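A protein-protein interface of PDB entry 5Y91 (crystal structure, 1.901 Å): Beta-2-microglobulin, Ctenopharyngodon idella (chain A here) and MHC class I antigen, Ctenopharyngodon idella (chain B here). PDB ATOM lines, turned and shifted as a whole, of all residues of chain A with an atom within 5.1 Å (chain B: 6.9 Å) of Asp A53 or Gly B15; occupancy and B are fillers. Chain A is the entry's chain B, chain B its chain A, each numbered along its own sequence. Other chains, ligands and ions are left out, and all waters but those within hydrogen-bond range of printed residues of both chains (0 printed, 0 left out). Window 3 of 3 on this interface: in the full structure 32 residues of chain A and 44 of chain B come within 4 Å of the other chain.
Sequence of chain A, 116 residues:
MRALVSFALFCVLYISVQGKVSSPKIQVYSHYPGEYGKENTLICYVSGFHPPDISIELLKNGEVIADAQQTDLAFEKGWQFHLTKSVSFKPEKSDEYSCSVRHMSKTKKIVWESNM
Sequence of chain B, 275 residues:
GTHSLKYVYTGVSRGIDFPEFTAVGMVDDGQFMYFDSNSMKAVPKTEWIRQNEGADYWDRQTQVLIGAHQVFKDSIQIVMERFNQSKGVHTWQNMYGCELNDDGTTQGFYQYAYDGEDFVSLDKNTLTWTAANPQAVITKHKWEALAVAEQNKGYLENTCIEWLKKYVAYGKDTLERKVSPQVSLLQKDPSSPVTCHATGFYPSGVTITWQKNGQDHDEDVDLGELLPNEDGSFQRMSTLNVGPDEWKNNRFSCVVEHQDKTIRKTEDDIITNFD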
ATOM      1  N   PRO A  51     -22.577   2.679  34.126  1.00  0.00           N
ATOM      2  CA  PRO A  51     -22.214   3.314  32.851  1.00  0.00           C
ATOM      3  C   PRO A  51     -22.595   4.797  32.786  1.00  0.00           C
ATOM      4  O   PRO A  51     -23.275   5.290  33.687  1.00  0.00           O
ATOM      5  CB  PRO A  51     -23.022   2.509  31.823  1.00  0.00           C
ATOM      6  CG  PRO A  51     -24.148   1.921  32.597  1.00  0.00           C
ATOM      7  CD  PRO A  51     -23.574   1.611  33.939  1.00  0.00           C
ATOM      8  N   PRO A  52     -22.157   5.500  31.727  1.00  0.00           N
ATOM      9  CA  PRO A  52     -22.345   6.953  31.591  1.00  0.00           C
ATOM     10  C   PRO A  52     -23.776   7.399  31.285  1.00  0.00           C
ATOM     11  O   PRO A  52     -24.122   8.538  31.603  1.00  0.00           O
ATOM     12  CB  PRO A  52     -21.422   7.314  30.423  1.00  0.00           C
ATOM     13  CG  PRO A  52     -21.310   6.058  29.634  1.00  0.00           C
ATOM     14  CD  PRO A  52     -21.315   4.956  30.647  1.00  0.00           C
ATOM     15  N   ASP A  53     -24.589   6.542  30.676  1.00  0.00           N
ATOM     16  CA  ASP A  53     -25.975   6.907  30.387  1.00  0.00           C
ATOM     17  C   ASP A  53     -26.700   7.323  31.664  1.00  0.00           C
ATOM     18  O   ASP A  53     -26.827   6.540  32.604  1.00  0.00           O
ATOM     19  CB  ASP A  53     -26.720   5.766  29.692  1.00  0.00           C
ATOM     20  CG  ASP A  53     -26.673   5.875  28.174  1.00  0.00           C
ATOM     21  OD1 ASP A  53     -27.433   5.148  27.501  1.00  0.00           O
ATOM     22  OD2 ASP A  53     -25.881   6.691  27.655  1.00  0.00           O
ATOM     23  N   ILE A  54     -27.177   8.561  31.691  1.00  0.00           N
ATOM     24  CA  ILE A  54     -27.754   9.122  32.905  1.00  0.00           C
ATOM     25  C   ILE A  54     -28.646  10.316  32.578  1.00  0.00           C
ATOM     26  O   ILE A  54     -28.517  10.927  31.517  1.00  0.00           O
ATOM     27  CB  ILE A  54     -26.640   9.547  33.881  1.00  0.00           C
ATOM     28  CG1 ILE A  54     -27.204   9.844  35.271  1.00  0.00           C
ATOM     29  CG2 ILE A  54     -25.874  10.741  33.330  1.00  0.00           C
ATOM     30  CD1 ILE A  54     -26.137   9.920  36.339  1.00  0.00           C
ATOM     31  N   SER A  55     -29.558  10.634  33.489  1.00  0.00           N
ATOM     32  CA  SER A  55     -30.451  11.771  33.315  1.00  0.00           C
ATOM     33  C   SER A  55     -30.407  12.653  34.553  1.00  0.00           C
ATOM     34  O   SER A  55     -30.624  12.179  35.665  1.00  0.00           O
ATOM     35  CB  SER A  55     -31.883  11.293  33.064  1.00  0.00           C
ATOM     36  OG  SER A  55     -32.794  12.378  33.063  1.00  0.00           O
ATOM     37  N   ARG A 102     -31.637  10.111  37.288  1.00  0.00           N
ATOM     38  CA  ARG A 102     -32.025   8.756  36.924  1.00  0.00           C
ATOM     39  C   ARG A 102     -30.826   8.026  36.326  1.00  0.00           C
ATOM     40  O   ARG A 102     -30.265   8.454  35.315  1.00  0.00           O
ATOM     41  CB  ARG A 102     -33.199   8.782  35.938  1.00  0.00           C
ATOM     42  CG  ARG A 102     -33.643   7.404  35.454  1.00  0.00           C
ATOM     43  CD  ARG A 102     -34.045   7.425  33.996  1.00  0.00           C
ATOM     44  NE  ARG A 102     -32.945   7.837  33.134  1.00  0.00           N
ATOM     45  CZ  ARG A 102     -32.088   6.995  32.570  1.00  0.00           C
ATOM     46  NH1 ARG A 102     -32.194   5.692  32.782  1.00  0.00           N
ATOM     47  NH2 ARG A 102     -31.123   7.456  31.793  1.00  0.00           N
ATOM     48  N   HIS A 103     -30.425   6.935  36.970  1.00  0.00           N
ATOM     49  CA  HIS A 103     -29.316   6.125  36.488  1.00  0.00           C
ATOM     50  C   HIS A 103     -29.722   4.659  36.507  1.00  0.00           C
ATOM     51  O   HIS A 103     -29.959   4.086  37.572  1.00  0.00           O
ATOM     52  CB  HIS A 103     -28.079   6.352  37.353  1.00  0.00           C
ATOM     53  CG  HIS A 103     -26.849   5.672  36.839  1.00  0.00           C
ATOM     54  ND1 HIS A 103     -26.193   4.688  37.548  1.00  0.00           N
ATOM     55  CD2 HIS A 103     -26.156   5.829  35.688  1.00  0.00           C
ATOM     56  CE1 HIS A 103     -25.146   4.274  36.857  1.00  0.00           C
ATOM     57  NE2 HIS A 103     -25.102   4.949  35.722  1.00  0.00           N
ATOM     58  N   MET A 104     -29.813   4.065  35.321  1.00  0.00           N
ATOM     59  CA  MET A 104     -30.261   2.686  35.186  1.00  0.00           C
ATOM     60  C   MET A 104     -31.587   2.742  35.937  1.00  0.00           C
ATOM     61  O   MET A 104     -32.362   3.685  35.771  1.00  0.00           O
ATOM     62  CB  MET A 104     -29.311   1.735  35.918  1.00  0.00           C
ATOM     63  CG  MET A 104     -27.869   1.785  35.424  1.00  0.00           C
ATOM     64  SD  MET A 104     -27.552   0.833  33.920  1.00  0.00           S
ATOM     65  CE  MET A 104     -28.479   1.737  32.688  1.00  0.00           C
ATOM     66  N   VAL B  12     -18.672   4.739  23.676  1.00  0.00           N
ATOM     67  CA  VAL B  12     -19.838   4.019  24.151  1.00  0.00           C
ATOM     68  C   VAL B  12     -20.525   3.143  23.088  1.00  0.00           C
ATOM     69  O   VAL B  12     -20.697   3.560  22.006  1.00  0.00           O
ATOM     70  CB  VAL B  12     -20.855   5.000  24.746  1.00  0.00           C
ATOM     71  CG1 VAL B  12     -22.076   4.271  25.236  1.00  0.00           C
ATOM     72  CG2 VAL B  12     -20.282   5.778  25.882  1.00  0.00           C
ATOM     73  N   SER B  13     -20.917   1.939  23.498  1.00  0.00           N
ATOM     74  CA  SER B  13     -21.631   1.000  22.647  1.00  0.00           C
ATOM     75  C   SER B  13     -23.079   1.075  23.113  1.00  0.00           C
ATOM     76  O   SER B  13     -23.364   0.895  24.297  1.00  0.00           O
ATOM     77  CB  SER B  13     -21.084  -0.415  22.820  1.00  0.00           C
ATOM     78  OG  SER B  13     -20.324  -0.811  21.693  1.00  0.00           O
ATOM     79  N   ARG B  14     -23.993   1.355  22.191  1.00  0.00           N
ATOM     80  CA  ARG B  14     -25.423   1.499  22.543  1.00  0.00           C
ATOM     81  C   ARG B  14     -25.727   2.879  23.152  1.00  0.00           C
ATOM     82  O   ARG B  14     -25.047   3.331  24.030  1.00  0.00           O
ATOM     83  CB  ARG B  14     -25.952   0.440  23.472  1.00  0.00           C
ATOM     84  CG  ARG B  14     -25.284  -0.919  23.457  1.00  0.00           C
ATOM     85  CD  ARG B  14     -25.212  -1.534  22.094  1.00  0.00           C
ATOM     86  NE  ARG B  14     -25.954  -2.788  21.939  1.00  0.00           N
ATOM     87  CZ  ARG B  14     -25.401  -3.985  21.870  1.00  0.00           C
ATOM     88  NH1 ARG B  14     -24.102  -4.157  22.032  1.00  0.00           N
ATOM     89  NH2 ARG B  14     -26.154  -5.033  21.654  1.00  0.00           N
ATOM     90  N   GLY B  15     -26.780   3.541  22.656  1.00  0.00           N
ATOM     91  CA  GLY B  15     -27.131   4.883  23.091  1.00  0.00           C
ATOM     92  C   GLY B  15     -28.052   4.894  24.296  1.00  0.00           C
ATOM     93  O   GLY B  15     -28.028   3.971  25.111  1.00  0.00           O
ATOM     94  N   ILE B  16     -28.867   5.937  24.413  1.00  0.00           N
ATOM     95  CA  ILE B  16     -28.891   7.022  23.436  1.00  0.00           C
ATOM     96  C   ILE B  16     -28.300   8.297  24.026  1.00  0.00           C
ATOM     97  O   ILE B  16     -27.800   9.157  23.299  1.00  0.00           O
ATOM     98  CB  ILE B  16     -30.331   7.314  22.956  1.00  0.00           C
ATOM     99  CG1 ILE B  16     -30.479   6.988  21.469  1.00  0.00           C
ATOM    100  CG2 ILE B  16     -30.712   8.764  23.226  1.00  0.00           C
ATOM    101  CD1 ILE B  16     -30.489   5.509  21.164  1.00  0.00           C
ATOM    102  N   ASP B  17     -28.353   8.397  25.351  1.00  0.00           N
ATOM    103  CA  ASP B  17     -27.945   9.600  26.075  1.00  0.00           C
ATOM    104  C   ASP B  17     -26.731  10.314  25.480  1.00  0.00           C
ATOM    105  O   ASP B  17     -26.715  11.540  25.386  1.00  0.00           O
ATOM    106  CB  ASP B  17     -27.689   9.269  27.549  1.00  0.00           C
ATOM    107  CG  ASP B  17     -28.936   8.777  28.260  1.00  0.00           C
ATOM    108  OD1 ASP B  17     -28.803   8.062  29.274  1.00  0.00           O
ATOM    109  OD2 ASP B  17     -30.051   9.104  27.799  1.00  0.00           O
ATOM    110  N   PHE B  18     -25.719   9.549  25.081  1.00  0.00           N
ATOM    111  CA  PHE B  18     -24.495  10.135  24.545  1.00  0.00           C
ATOM    112  C   PHE B  18     -24.100   9.520  23.201  1.00  0.00           C
ATOM    113  O   PHE B  18     -24.496   8.398  22.884  1.00  0.00           O
ATOM    114  CB  PHE B  18     -23.350   9.993  25.554  1.00  0.00           C
ATOM    115  CG  PHE B  18     -23.599  10.696  26.861  1.00  0.00           C
ATOM    116  CD1 PHE B  18     -23.400  12.062  26.977  1.00  0.00           C
ATOM    117  CD2 PHE B  18     -24.026   9.989  27.975  1.00  0.00           C
ATOM    118  CE1 PHE B  18     -23.627  12.714  28.180  1.00  0.00           C
ATOM    119  CE2 PHE B  18     -24.256  10.633  29.183  1.00  0.00           C
ATOM    120  CZ  PHE B  18     -24.056  11.998  29.286  1.00  0.00           C
ATOM    121  N   PRO B  19     -23.323  10.266  22.401  1.00  0.00           N
ATOM    122  CA  PRO B  19     -22.809   9.782  21.114  1.00  0.00           C
ATOM    123  C   PRO B  19     -21.793   8.655  21.288  1.00  0.00           C
ATOM    124  O   PRO B  19     -21.353   8.391  22.407  1.00  0.00           O
ATOM    125  CB  PRO B  19     -22.122  11.019  20.521  1.00  0.00           C
ATOM    126  CG  PRO B  19     -21.869  11.919  21.681  1.00  0.00           C
ATOM    127  CD  PRO B  19     -23.003  11.685  22.622  1.00  0.00           C
ATOM    128  N   VAL B  89     -24.652  -2.560  26.960  1.00  0.00           N
ATOM    129  CA  VAL B  89     -24.037  -1.237  26.857  1.00  0.00           C
ATOM    130  C   VAL B  89     -22.687  -1.202  27.576  1.00  0.00           C
ATOM    131  O   VAL B  89     -22.598  -1.511  28.768  1.00  0.00           O
ATOM    132  CB  VAL B  89     -24.966  -0.141  27.407  1.00  0.00           C
ATOM    133  CG1 VAL B  89     -25.882  -0.709  28.481  1.00  0.00           C
ATOM    134  CG2 VAL B  89     -24.157   1.032  27.938  1.00  0.00           C
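Asp A53 touches four residues of chain B. Ser B13 touches none of the printed residues of chain A. Gly B15 touches one residue of chain A. Printed residues of chain A within 4 Å of Ile B16: Asp A53. Printed residues of chain A within 4 Å of Asp B17: Asp A53, Ile A54 and Arg A102. The nearest printed residue of chain A that does not touch Gly B15 is Met A104 (7.9 Å). The nearest printed residue of chain A that does not touch Phe B18 is Ile A54 (4.4 Å).
OD1 of Asp B17 lies within salt-bridge range of NH2 of Arg A102. The backbone NH (N) of Ile B16 is in hydrogen-bond range of the side-chain carboxylate (OD1) of Asp A53, at 3.5 Å. The side-chain carboxylate (OD1) of Asp A53 lies close to the backbone carbonyl oxygen (O) of Gly B15 (2.7 Å). OD1 of Asp B17 sits at hydrogen-bond distance from N of Ile A54 (3.0 Å).
N of Arg A102 lies within hydrogen-bond range of O of Ser A55 (2.8 Å).
Pro A52 touches Val B12 (CG to CG2, 3.9 Å). Pro A52 touches Phe B18 (O to CE2, 3.2 Å). CB of Asp A53 touches OD1 of Asp B17, at 3.1 Å. OD2 of Asp A53 touches CD2 of Phe B18, 3.8 Å away.
Printed residues of chain A that touch a printed residue of chain B: Pro A52, Asp A53, Ile A54 and Arg A102. Along chain A the printed residues that touch a printed residue of chain B span positions 52 to 102. Of the 9 printed residues of chain B, 5 touch a printed residue of chain A. Printed residues of chain B that touch a printed residue of chain A: Val B12, Gly B15, Ile B16, Asp B17 and Phe B18. Hydrophobic or aromatic side chains of chain B within 4 Å of the printed part of chain A: Val B12 and Phe B18. Among the printed residues, 8 pairs touch across the chains. Among the printed residues, Asp or Glu carboxylates within 4 Å of a Lys or Arg side-chain nitrogen of the other chain: Arg A102 with Asp B17.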
